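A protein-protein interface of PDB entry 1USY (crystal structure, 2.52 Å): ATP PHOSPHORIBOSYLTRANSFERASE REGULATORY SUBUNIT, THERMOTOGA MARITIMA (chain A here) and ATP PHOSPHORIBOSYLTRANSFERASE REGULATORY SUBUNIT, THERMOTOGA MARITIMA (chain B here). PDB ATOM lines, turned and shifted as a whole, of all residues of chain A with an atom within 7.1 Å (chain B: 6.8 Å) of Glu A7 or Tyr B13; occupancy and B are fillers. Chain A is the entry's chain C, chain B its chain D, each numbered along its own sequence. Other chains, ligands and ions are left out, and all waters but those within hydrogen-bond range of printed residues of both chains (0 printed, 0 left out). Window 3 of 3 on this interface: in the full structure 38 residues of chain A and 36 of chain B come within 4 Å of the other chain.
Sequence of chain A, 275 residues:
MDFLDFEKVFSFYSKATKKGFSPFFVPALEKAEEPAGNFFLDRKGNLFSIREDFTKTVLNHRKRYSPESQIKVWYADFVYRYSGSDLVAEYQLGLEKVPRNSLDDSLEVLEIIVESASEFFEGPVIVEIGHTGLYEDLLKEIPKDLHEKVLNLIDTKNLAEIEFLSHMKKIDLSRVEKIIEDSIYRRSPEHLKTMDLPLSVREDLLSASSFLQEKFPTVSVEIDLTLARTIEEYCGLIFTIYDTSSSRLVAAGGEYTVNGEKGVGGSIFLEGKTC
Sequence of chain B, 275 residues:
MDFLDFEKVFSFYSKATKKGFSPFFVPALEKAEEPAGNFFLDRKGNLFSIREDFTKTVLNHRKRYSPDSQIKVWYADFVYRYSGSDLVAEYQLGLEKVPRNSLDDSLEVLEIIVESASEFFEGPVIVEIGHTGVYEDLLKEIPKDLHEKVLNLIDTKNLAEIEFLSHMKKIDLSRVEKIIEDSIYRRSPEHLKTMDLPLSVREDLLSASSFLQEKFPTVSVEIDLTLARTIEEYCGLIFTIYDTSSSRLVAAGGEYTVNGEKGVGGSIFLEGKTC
Printed residues of chain B within 4 Å of Leu A4: Pro B23 (3.0 Å). Printed residues of chain B within 4 Å of Phe A6: Phe B10 (3.6 Å), Tyr B13 (3.4 Å) and Trp B74 (3.7 Å). Glu A7 touches just one residue of chain B: Tyr B13. Of the printed residues of chain B, Tyr A13 touches Phe B10. Of the printed residues of chain A, Phe B10 touches Phe A6 (3.6 Å), Phe A10 (3.4 Å) and Tyr A13 (3.4 Å). Of chain A, only Phe A6 and Glu A7 come within 4 Å of Tyr B13. Thr B17 touches none of the printed residues of chain A. Of the printed residues of chain A, Pro B23 touches Phe A3 and Leu A4. The nearest residue of chain A that does not touch Tyr B13 is Phe A10 (4.6 Å).
O of Tyr B13 lies close to OG1 of Thr B17, at 3.5 Å. The backbone carbonyl oxygen (O) of Phe A10 is in hydrogen-bond range of the side-chain hydroxyl (OG) of Ser A14, at 3.0 Å.
O of Pro B23 touches CA of Phe A3, at 3.5 Å. CG of Pro B23 touches O of Leu A4, at 3.0 Å. CE1 of Phe B10 touches CE1 of Phe A6 (3.6 Å). CD1 of Phe A6 touches CD1 of Tyr B13, 3.4 Å away. CZ2 of Trp B74 touches CD1 of Phe A6, at 3.7 Å. N of Glu A7 touches OH of Tyr B13, 3.8 Å away. Phe B10 touches Phe A10 (CD1 to CD1, 3.4 Å). Phe B10 touches Tyr A13 (CE2 to CG, 3.4 Å).
Printed residues of chain A that touch a printed residue of chain B: Phe A3, Leu A4, Phe A6, Glu A7, Phe A10 and Tyr A13. Hydrophobic or aromatic side chains of chain A that line the printed part of chain B: Phe A3, Phe A6, Phe A10 and Tyr A13. Of the 15 printed residues of chain B, 4 touch a printed residue of chain A. Printed residues of chain B that touch a printed residue of chain A: Phe B10, Tyr B13, Pro B23 and Trp B74.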
ATOM      1  N   PHE A   3      21.524   9.230   6.177  1.00  0.00           N
ATOM      2  CA  PHE A   3      21.102   8.608   7.415  1.00  0.00           C
ATOM      3  C   PHE A   3      22.194   8.873   8.439  1.00  0.00           C
ATOM      4  O   PHE A   3      23.365   9.050   8.087  1.00  0.00           O
ATOM      5  CB  PHE A   3      20.930   7.096   7.177  1.00  0.00           C
ATOM      6  CG  PHE A   3      20.460   6.328   8.383  1.00  0.00           C
ATOM      7  CD1 PHE A   3      19.097   6.180   8.630  1.00  0.00           C
ATOM      8  CD2 PHE A   3      21.378   5.707   9.249  1.00  0.00           C
ATOM      9  CE1 PHE A   3      18.649   5.479   9.743  1.00  0.00           C
ATOM     10  CE2 PHE A   3      20.931   4.998  10.350  1.00  0.00           C
ATOM     11  CZ  PHE A   3      19.547   4.888  10.594  1.00  0.00           C
ATOM     12  N   LEU A   4      21.787   8.929   9.687  1.00  0.00           N
ATOM     13  CA  LEU A   4      22.685   8.977  10.818  1.00  0.00           C
ATOM     14  C   LEU A   4      22.090   8.056  11.899  1.00  0.00           C
ATOM     15  O   LEU A   4      20.912   8.159  12.250  1.00  0.00           O
ATOM     16  CB  LEU A   4      22.801  10.403  11.338  1.00  0.00           C
ATOM     17  CG  LEU A   4      23.804  10.506  12.476  1.00  0.00           C
ATOM     18  CD1 LEU A   4      25.047  11.225  11.994  1.00  0.00           C
ATOM     19  CD2 LEU A   4      23.223  11.204  13.690  1.00  0.00           C
ATOM     20  N   ASP A   5      22.895   7.124  12.378  1.00  0.00           N
ATOM     21  CA  ASP A   5      22.485   6.255  13.476  1.00  0.00           C
ATOM     22  C   ASP A   5      22.258   7.101  14.736  1.00  0.00           C
ATOM     23  O   ASP A   5      23.172   7.297  15.542  1.00  0.00           O
ATOM     24  CB  ASP A   5      23.552   5.204  13.718  1.00  0.00           C
ATOM     25  CG  ASP A   5      23.051   4.041  14.517  1.00  0.00           C
ATOM     26  OD1 ASP A   5      23.802   3.037  14.592  1.00  0.00           O
ATOM     27  OD2 ASP A   5      21.935   4.025  15.102  1.00  0.00           O
ATOM     28  N   PHE A   6      21.034   7.606  14.876  1.00  0.00           N
ATOM     29  CA  PHE A   6      20.728   8.610  15.881  1.00  0.00           C
ATOM     30  C   PHE A   6      20.486   8.028  17.264  1.00  0.00           C
ATOM     31  O   PHE A   6      20.623   8.747  18.256  1.00  0.00           O
ATOM     32  CB  PHE A   6      19.596   9.545  15.425  1.00  0.00           C
ATOM     33  CG  PHE A   6      19.562  10.831  16.176  1.00  0.00           C
ATOM     34  CD1 PHE A   6      18.606  11.033  17.190  1.00  0.00           C
ATOM     35  CD2 PHE A   6      20.500  11.846  15.920  1.00  0.00           C
ATOM     36  CE1 PHE A   6      18.588  12.222  17.939  1.00  0.00           C
ATOM     37  CE2 PHE A   6      20.470  13.068  16.680  1.00  0.00           C
ATOM     38  CZ  PHE A   6      19.514  13.222  17.683  1.00  0.00           C
ATOM     39  N   GLU A   7      20.176   6.726  17.332  1.00  0.00           N
ATOM     40  CA  GLU A   7      20.052   6.017  18.620  1.00  0.00           C
ATOM     41  C   GLU A   7      21.358   6.116  19.377  1.00  0.00           C
ATOM     42  O   GLU A   7      21.378   6.276  20.605  1.00  0.00           O
ATOM     43  CB  GLU A   7      19.686   4.548  18.429  1.00  0.00           C
ATOM     44  CG  GLU A   7      18.433   4.110  19.169  1.00  0.00           C
ATOM     45  CD  GLU A   7      18.302   2.585  19.274  1.00  0.00           C
ATOM     46  OE1 GLU A   7      17.742   1.944  18.340  1.00  0.00           O
ATOM     47  OE2 GLU A   7      18.753   2.018  20.301  1.00  0.00           O
ATOM     48  N   LYS A   8      22.458   6.032  18.633  1.00  0.00           N
ATOM     49  CA  LYS A   8      23.788   6.109  19.239  1.00  0.00           C
ATOM     50  C   LYS A   8      23.943   7.462  19.864  1.00  0.00           C
ATOM     51  O   LYS A   8      24.395   7.544  20.998  1.00  0.00           O
ATOM     52  CB  LYS A   8      24.904   5.817  18.237  1.00  0.00           C
ATOM     53  CG  LYS A   8      24.923   4.350  17.773  1.00  0.00           C
ATOM     54  CD  LYS A   8      25.963   4.156  16.673  1.00  0.00           C
ATOM     55  CE  LYS A   8      26.637   2.816  16.759  1.00  0.00           C
ATOM     56  NZ  LYS A   8      25.727   1.728  16.411  1.00  0.00           N
ATOM     57  N   VAL A   9      23.492   8.520  19.181  1.00  0.00           N
ATOM     58  CA  VAL A   9      23.580   9.865  19.785  1.00  0.00           C
ATOM     59  C   VAL A   9      22.726   9.937  21.068  1.00  0.00           C
ATOM     60  O   VAL A   9      23.168  10.450  22.109  1.00  0.00           O
ATOM     61  CB  VAL A   9      23.185  11.014  18.845  1.00  0.00           C
ATOM     62  CG1 VAL A   9      23.548  12.334  19.472  1.00  0.00           C
ATOM     63  CG2 VAL A   9      23.858  10.879  17.494  1.00  0.00           C
ATOM     64  N   PHE A  10      21.523   9.374  20.991  1.00  0.00           N
ATOM     65  CA  PHE A  10      20.656   9.279  22.152  1.00  0.00           C
ATOM     66  C   PHE A  10      21.362   8.545  23.308  1.00  0.00           C
ATOM     67  O   PHE A  10      21.352   9.007  24.457  1.00  0.00           O
ATOM     68  CB  PHE A  10      19.303   8.627  21.798  1.00  0.00           C
ATOM     69  CG  PHE A  10      18.348   8.622  22.926  1.00  0.00           C
ATOM     70  CD1 PHE A  10      17.757   9.809  23.338  1.00  0.00           C
ATOM     71  CD2 PHE A  10      18.094   7.447  23.635  1.00  0.00           C
ATOM     72  CE1 PHE A  10      16.895   9.834  24.443  1.00  0.00           C
ATOM     73  CE2 PHE A  10      17.215   7.450  24.731  1.00  0.00           C
ATOM     74  CZ  PHE A  10      16.619   8.659  25.136  1.00  0.00           C
ATOM     75  N   SER A  11      22.027   7.440  22.977  1.00  0.00           N
ATOM     76  CA  SER A  11      22.601   6.559  23.991  1.00  0.00           C
ATOM     77  C   SER A  11      23.775   7.264  24.674  1.00  0.00           C
ATOM     78  O   SER A  11      23.890   7.248  25.917  1.00  0.00           O
ATOM     79  CB  SER A  11      22.969   5.195  23.382  1.00  0.00           C
ATOM     80  OG  SER A  11      23.749   4.440  24.286  1.00  0.00           O
ATOM     81  N   PHE A  12      24.586   7.930  23.859  1.00  0.00           N
ATOM     82  CA  PHE A  12      25.676   8.802  24.316  1.00  0.00           C
ATOM     83  C   PHE A  12      25.143   9.935  25.167  1.00  0.00           C
ATOM     84  O   PHE A  12      25.729  10.215  26.224  1.00  0.00           O
ATOM     85  CB  PHE A  12      26.406   9.383  23.119  1.00  0.00           C
ATOM     86  CG  PHE A  12      27.638  10.166  23.469  1.00  0.00           C
ATOM     87  CD1 PHE A  12      28.800   9.509  23.837  1.00  0.00           C
ATOM     88  CD2 PHE A  12      27.659  11.542  23.339  1.00  0.00           C
ATOM     89  CE1 PHE A  12      29.936  10.217  24.139  1.00  0.00           C
ATOM     90  CE2 PHE A  12      28.794  12.249  23.623  1.00  0.00           C
ATOM     91  CZ  PHE A  12      29.940  11.582  24.029  1.00  0.00           C
ATOM     92  N   TYR A  13      24.009  10.532  24.751  1.00  0.00           N
ATOM     93  CA  TYR A  13      23.378  11.588  25.540  1.00  0.00           C
ATOM     94  C   TYR A  13      22.975  11.016  26.908  1.00  0.00           C
ATOM     95  O   TYR A  13      23.285  11.592  27.948  1.00  0.00           O
ATOM     96  CB  TYR A  13      22.191  12.235  24.772  1.00  0.00           C
ATOM     97  CG  TYR A  13      21.044  12.839  25.620  1.00  0.00           C
ATOM     98  CD1 TYR A  13      21.169  14.096  26.213  1.00  0.00           C
ATOM     99  CD2 TYR A  13      19.814  12.172  25.771  1.00  0.00           C
ATOM    100  CE1 TYR A  13      20.114  14.678  26.945  1.00  0.00           C
ATOM    101  CE2 TYR A  13      18.765  12.744  26.528  1.00  0.00           C
ATOM    102  CZ  TYR A  13      18.932  14.009  27.105  1.00  0.00           C
ATOM    103  OH  TYR A  13      17.942  14.618  27.857  1.00  0.00           O
ATOM    104  N   SER A  14      22.321   9.862  26.904  1.00  0.00           N
ATOM    105  CA  SER A  14      21.853   9.276  28.153  1.00  0.00           C
ATOM    106  C   SER A  14      23.033   8.982  29.093  1.00  0.00           C
ATOM    107  O   SER A  14      22.920   9.157  30.306  1.00  0.00           O
ATOM    108  CB  SER A  14      20.993   8.014  27.931  1.00  0.00           C
ATOM    109  OG  SER A  14      19.964   8.271  26.986  1.00  0.00           O
ATOM    110  N   GLU A 119      29.950  -0.460  23.182  1.00  0.00           N
ATOM    111  CA  GLU A 119      28.543  -0.657  22.910  1.00  0.00           C
ATOM    112  C   GLU A 119      28.237  -0.452  21.442  1.00  0.00           C
ATOM    113  O   GLU A 119      27.376  -1.128  20.931  1.00  0.00           O
ATOM    114  CB  GLU A 119      27.763   0.358  23.702  1.00  0.00           C
ATOM    115  CG  GLU A 119      26.264   0.281  23.556  1.00  0.00           C
ATOM    116  CD  GLU A 119      25.564   1.142  24.598  1.00  0.00           C
ATOM    117  OE1 GLU A 119      25.865   0.959  25.815  1.00  0.00           O
ATOM    118  OE2 GLU A 119      24.730   1.989  24.190  1.00  0.00           O
ATOM    119  N   PHE A 120      28.924   0.506  20.804  1.00  0.00           N
ATOM    120  CA  PHE A 120      28.759   0.869  19.399  1.00  0.00           C
ATOM    121  C   PHE A 120      29.541   0.003  18.397  1.00  0.00           C
ATOM    122  O   PHE A 120      29.201  -0.015  17.228  1.00  0.00           O
ATOM    123  CB  PHE A 120      29.225   2.301  19.180  1.00  0.00           C
ATOM    124  CG  PHE A 120      28.431   3.337  19.933  1.00  0.00           C
ATOM    125  CD1 PHE A 120      28.913   4.648  20.001  1.00  0.00           C
ATOM    126  CD2 PHE A 120      27.204   3.015  20.584  1.00  0.00           C
ATOM    127  CE1 PHE A 120      28.207   5.638  20.697  1.00  0.00           C
ATOM    128  CE2 PHE A 120      26.487   4.018  21.280  1.00  0.00           C
ATOM    129  CZ  PHE A 120      27.009   5.340  21.328  1.00  0.00           C
ATOM    130  N   LYS B   8      15.093  19.129  23.636  1.00  0.00           N
ATOM    131  CA  LYS B   8      13.789  18.968  22.974  1.00  0.00           C
ATOM    132  C   LYS B   8      13.912  18.178  21.659  1.00  0.00           C
ATOM    133  O   LYS B   8      12.909  17.752  21.072  1.00  0.00           O
ATOM    134  CB  LYS B   8      13.167  20.339  22.686  1.00  0.00           C
ATOM    135  CG  LYS B   8      12.860  21.131  23.945  1.00  0.00           C
ATOM    136  CD  LYS B   8      12.535  22.591  23.637  1.00  0.00           C
ATOM    137  CE  LYS B   8      12.131  23.291  24.927  1.00  0.00           C
ATOM    138  NZ  LYS B   8      11.951  24.737  24.776  1.00  0.00           N
ATOM    139  N   VAL B   9      15.164  17.984  21.233  1.00  0.00           N
ATOM    140  CA  VAL B   9      15.521  17.312  19.994  1.00  0.00           C
ATOM    141  C   VAL B   9      15.236  15.810  20.065  1.00  0.00           C
ATOM    142  O   VAL B   9      14.838  15.185  19.064  1.00  0.00           O
ATOM    143  CB  VAL B   9      16.993  17.548  19.697  1.00  0.00           C
ATOM    144  CG1 VAL B   9      17.408  16.884  18.389  1.00  0.00           C
ATOM    145  CG2 VAL B   9      17.230  19.036  19.603  1.00  0.00           C
ATOM    146  N   PHE B  10      15.428  15.245  21.254  1.00  0.00           N
ATOM    147  CA  PHE B  10      15.234  13.824  21.476  1.00  0.00           C
ATOM    148  C   PHE B  10      13.745  13.554  21.541  1.00  0.00           C
ATOM    149  O   PHE B  10      13.262  12.534  21.040  1.00  0.00           O
ATOM    150  CB  PHE B  10      16.032  13.342  22.719  1.00  0.00           C
ATOM    151  CG  PHE B  10      17.523  13.478  22.539  1.00  0.00           C
ATOM    152  CD1 PHE B  10      18.185  12.729  21.565  1.00  0.00           C
ATOM    153  CD2 PHE B  10      18.263  14.412  23.282  1.00  0.00           C
ATOM    154  CE1 PHE B  10      19.566  12.891  21.350  1.00  0.00           C
ATOM    155  CE2 PHE B  10      19.661  14.589  23.075  1.00  0.00           C
ATOM    156  CZ  PHE B  10      20.298  13.835  22.103  1.00  0.00           C
ATOM    157  N   SER B  11      13.019  14.494  22.135  1.00  0.00           N
ATOM    158  CA  SER B  11      11.566  14.481  22.130  1.00  0.00           C
ATOM    159  C   SER B  11      11.067  14.520  20.658  1.00  0.00           C
ATOM    160  O   SER B  11      10.222  13.692  20.231  1.00  0.00           O
ATOM    161  CB  SER B  11      11.062  15.678  22.916  1.00  0.00           C
ATOM    162  OG  SER B  11       9.674  15.609  23.060  1.00  0.00           O
ATOM    163  N   PHE B  12      11.629  15.436  19.877  1.00  0.00           N
ATOM    164  CA  PHE B  12      11.246  15.589  18.480  1.00  0.00           C
ATOM    165  C   PHE B  12      11.596  14.352  17.675  1.00  0.00           C
ATOM    166  O   PHE B  12      10.800  13.875  16.819  1.00  0.00           O
ATOM    167  CB  PHE B  12      11.977  16.771  17.894  1.00  0.00           C
ATOM    168  CG  PHE B  12      11.613  17.069  16.495  1.00  0.00           C
ATOM    169  CD1 PHE B  12      10.400  17.684  16.195  1.00  0.00           C
ATOM    170  CD2 PHE B  12      12.504  16.790  15.470  1.00  0.00           C
ATOM    171  CE1 PHE B  12      10.075  17.998  14.877  1.00  0.00           C
ATOM    172  CE2 PHE B  12      12.186  17.079  14.167  1.00  0.00           C
ATOM    173  CZ  PHE B  12      10.980  17.683  13.859  1.00  0.00           C
ATOM    174  N   TYR B  13      12.781  13.819  17.984  1.00  0.00           N
ATOM    175  CA  TYR B  13      13.257  12.596  17.379  1.00  0.00           C
ATOM    176  C   TYR B  13      12.261  11.460  17.643  1.00  0.00           C
ATOM    177  O   TYR B  13      11.967  10.684  16.733  1.00  0.00           O
ATOM    178  CB  TYR B  13      14.684  12.280  17.852  1.00  0.00           C
ATOM    179  CG  TYR B  13      15.126  10.823  17.746  1.00  0.00           C
ATOM    180  CD1 TYR B  13      15.327  10.220  16.492  1.00  0.00           C
ATOM    181  CD2 TYR B  13      15.368  10.046  18.895  1.00  0.00           C
ATOM    182  CE1 TYR B  13      15.742   8.880  16.385  1.00  0.00           C
ATOM    183  CE2 TYR B  13      15.766   8.704  18.787  1.00  0.00           C
ATOM    184  CZ  TYR B  13      15.957   8.145  17.520  1.00  0.00           C
ATOM    185  OH  TYR B  13      16.364   6.846  17.384  1.00  0.00           O
ATOM    186  N   SER B  14      11.705  11.392  18.855  1.00  0.00           N
ATOM    187  CA  SER B  14      10.746  10.345  19.170  1.00  0.00           C
ATOM    188  C   SER B  14       9.458  10.491  18.380  1.00  0.00           C
ATOM    189  O   SER B  14       9.003   9.523  17.757  1.00  0.00           O
ATOM    190  CB  SER B  14      10.432  10.270  20.667  1.00  0.00           C
ATOM    191  OG  SER B  14      11.298   9.350  21.288  1.00  0.00           O
ATOM    192  N   LYS B  15       8.871  11.691  18.408  1.00  0.00           N
ATOM    193  CA  LYS B  15       7.655  11.965  17.655  1.00  0.00           C
ATOM    194  C   LYS B  15       7.858  11.469  16.219  1.00  0.00           C
ATOM    195  O   LYS B  15       7.043  10.684  15.727  1.00  0.00           O
ATOM    196  CB  LYS B  15       7.356  13.458  17.643  1.00  0.00           C
ATOM    197  CG  LYS B  15       6.449  13.968  18.742  1.00  0.00           C
ATOM    198  CD  LYS B  15       7.216  14.697  19.834  1.00  0.00           C
ATOM    199  CE  LYS B  15       6.407  15.778  20.512  1.00  0.00           C
ATOM    200  NZ  LYS B  15       5.520  15.174  21.582  1.00  0.00           N
ATOM    201  N   ALA B  16       8.973  11.875  15.583  1.00  0.00           N
ATOM    202  CA  ALA B  16       9.160  11.666  14.143  1.00  0.00           C
ATOM    203  C   ALA B  16       9.481  10.220  13.765  1.00  0.00           C
ATOM    204  O   ALA B  16       9.002   9.720  12.732  1.00  0.00           O
ATOM    205  CB  ALA B  16      10.202  12.637  13.559  1.00  0.00           C
ATOM    206  N   THR B  17      10.257   9.524  14.598  1.00  0.00           N
ATOM    207  CA  THR B  17      10.481   8.129  14.303  1.00  0.00           C
ATOM    208  C   THR B  17       9.219   7.236  14.478  1.00  0.00           C
ATOM    209  O   THR B  17       9.080   6.212  13.795  1.00  0.00           O
ATOM    210  CB  THR B  17      11.802   7.535  14.930  1.00  0.00           C
ATOM    211  OG1 THR B  17      11.652   7.243  16.316  1.00  0.00           O
ATOM    212  CG2 THR B  17      12.903   8.553  14.893  1.00  0.00           C
ATOM    213  N   LYS B  18       8.288   7.628  15.343  1.00  0.00           N
ATOM    214  CA  LYS B  18       7.112   6.785  15.560  1.00  0.00           C
ATOM    215  C   LYS B  18       6.213   6.927  14.356  1.00  0.00           C
ATOM    216  O   LYS B  18       5.351   6.080  14.090  1.00  0.00           O
ATOM    217  CB  LYS B  18       6.402   7.100  16.879  1.00  0.00           C
ATOM    218  CG  LYS B  18       7.326   6.825  18.098  1.00  0.00           C
ATOM    219  CD  LYS B  18       6.568   6.514  19.375  1.00  0.00           C
ATOM    220  CE  LYS B  18       6.158   7.789  20.078  1.00  0.00           C
ATOM    221  NZ  LYS B  18       5.641   7.518  21.445  1.00  0.00           N
ATOM    222  N   PHE B  21       9.777   8.679  10.222  1.00  0.00           N
ATOM    223  CA  PHE B  21      10.798   9.652   9.768  1.00  0.00           C
ATOM    224  C   PHE B  21      12.201   9.189  10.146  1.00  0.00           C
ATOM    225  O   PHE B  21      12.480   8.873  11.318  1.00  0.00           O
ATOM    226  CB  PHE B  21      10.533  11.079  10.302  1.00  0.00           C
ATOM    227  CG  PHE B  21       9.265  11.689   9.778  1.00  0.00           C
ATOM    228  CD1 PHE B  21       8.047  11.401  10.379  1.00  0.00           C
ATOM    229  CD2 PHE B  21       9.283  12.548   8.659  1.00  0.00           C
ATOM    230  CE1 PHE B  21       6.841  11.946   9.877  1.00  0.00           C
ATOM    231  CE2 PHE B  21       8.093  13.091   8.148  1.00  0.00           C
ATOM    232  CZ  PHE B  21       6.865  12.785   8.768  1.00  0.00           C
ATOM    233  N   PRO B  23      16.357   9.902  10.266  1.00  0.00           N
ATOM    234  CA  PRO B  23      17.153  11.098  10.542  1.00  0.00           C
ATOM    235  C   PRO B  23      17.929  11.498   9.312  1.00  0.00           C
ATOM    236  O   PRO B  23      18.603  10.667   8.700  1.00  0.00           O
ATOM    237  CB  PRO B  23      18.106  10.645  11.646  1.00  0.00           C
ATOM    238  CG  PRO B  23      18.204   9.136  11.463  1.00  0.00           C
ATOM    239  CD  PRO B  23      16.889   8.675  10.899  1.00  0.00           C
ATOM    240  N   TRP B  74      13.433  13.526   9.066  1.00  0.00           N
ATOM    241  CA  TRP B  74      13.478  14.612  10.001  1.00  0.00           C
ATOM    242  C   TRP B  74      14.879  15.137  10.118  1.00  0.00           C
ATOM    243  O   TRP B  74      15.831  14.376   9.983  1.00  0.00           O
ATOM    244  CB  TRP B  74      12.996  14.147  11.359  1.00  0.00           C
ATOM    245  CG  TRP B  74      13.910  13.225  12.099  1.00  0.00           C
ATOM    246  CD1 TRP B  74      13.881  11.840  12.078  1.00  0.00           C
ATOM    247  CD2 TRP B  74      14.940  13.587  13.020  1.00  0.00           C
ATOM    248  NE1 TRP B  74      14.838  11.332  12.926  1.00  0.00           N
ATOM    249  CE2 TRP B  74      15.509  12.377  13.513  1.00  0.00           C
ATOM    250  CE3 TRP B  74      15.443  14.809  13.494  1.00  0.00           C
ATOM    251  CZ2 TRP B  74      16.562  12.360  14.456  1.00  0.00           C
ATOM    252  CZ3 TRP B  74      16.503  14.798  14.425  1.00  0.00           C
ATOM    253  CH2 TRP B  74      17.048  13.578  14.893  1.00  0.00           C
ATOM    254  N   LEU B  93      14.344  22.318  13.820  1.00  0.00           N
ATOM    255  CA  LEU B  93      13.922  20.940  13.809  1.00  0.00           C
ATOM    256  C   LEU B  93      12.846  20.901  12.752  1.00  0.00           C
ATOM    257  O   LEU B  93      11.970  21.756  12.737  1.00  0.00           O
ATOM    258  CB  LEU B  93      13.298  20.528  15.139  1.00  0.00           C
ATOM    259  CG  LEU B  93      14.087  20.591  16.446  1.00  0.00           C
ATOM    260  CD1 LEU B  93      13.143  20.626  17.652  1.00  0.00           C
ATOM    261  CD2 LEU B  93      14.888  19.355  16.538  1.00  0.00           C
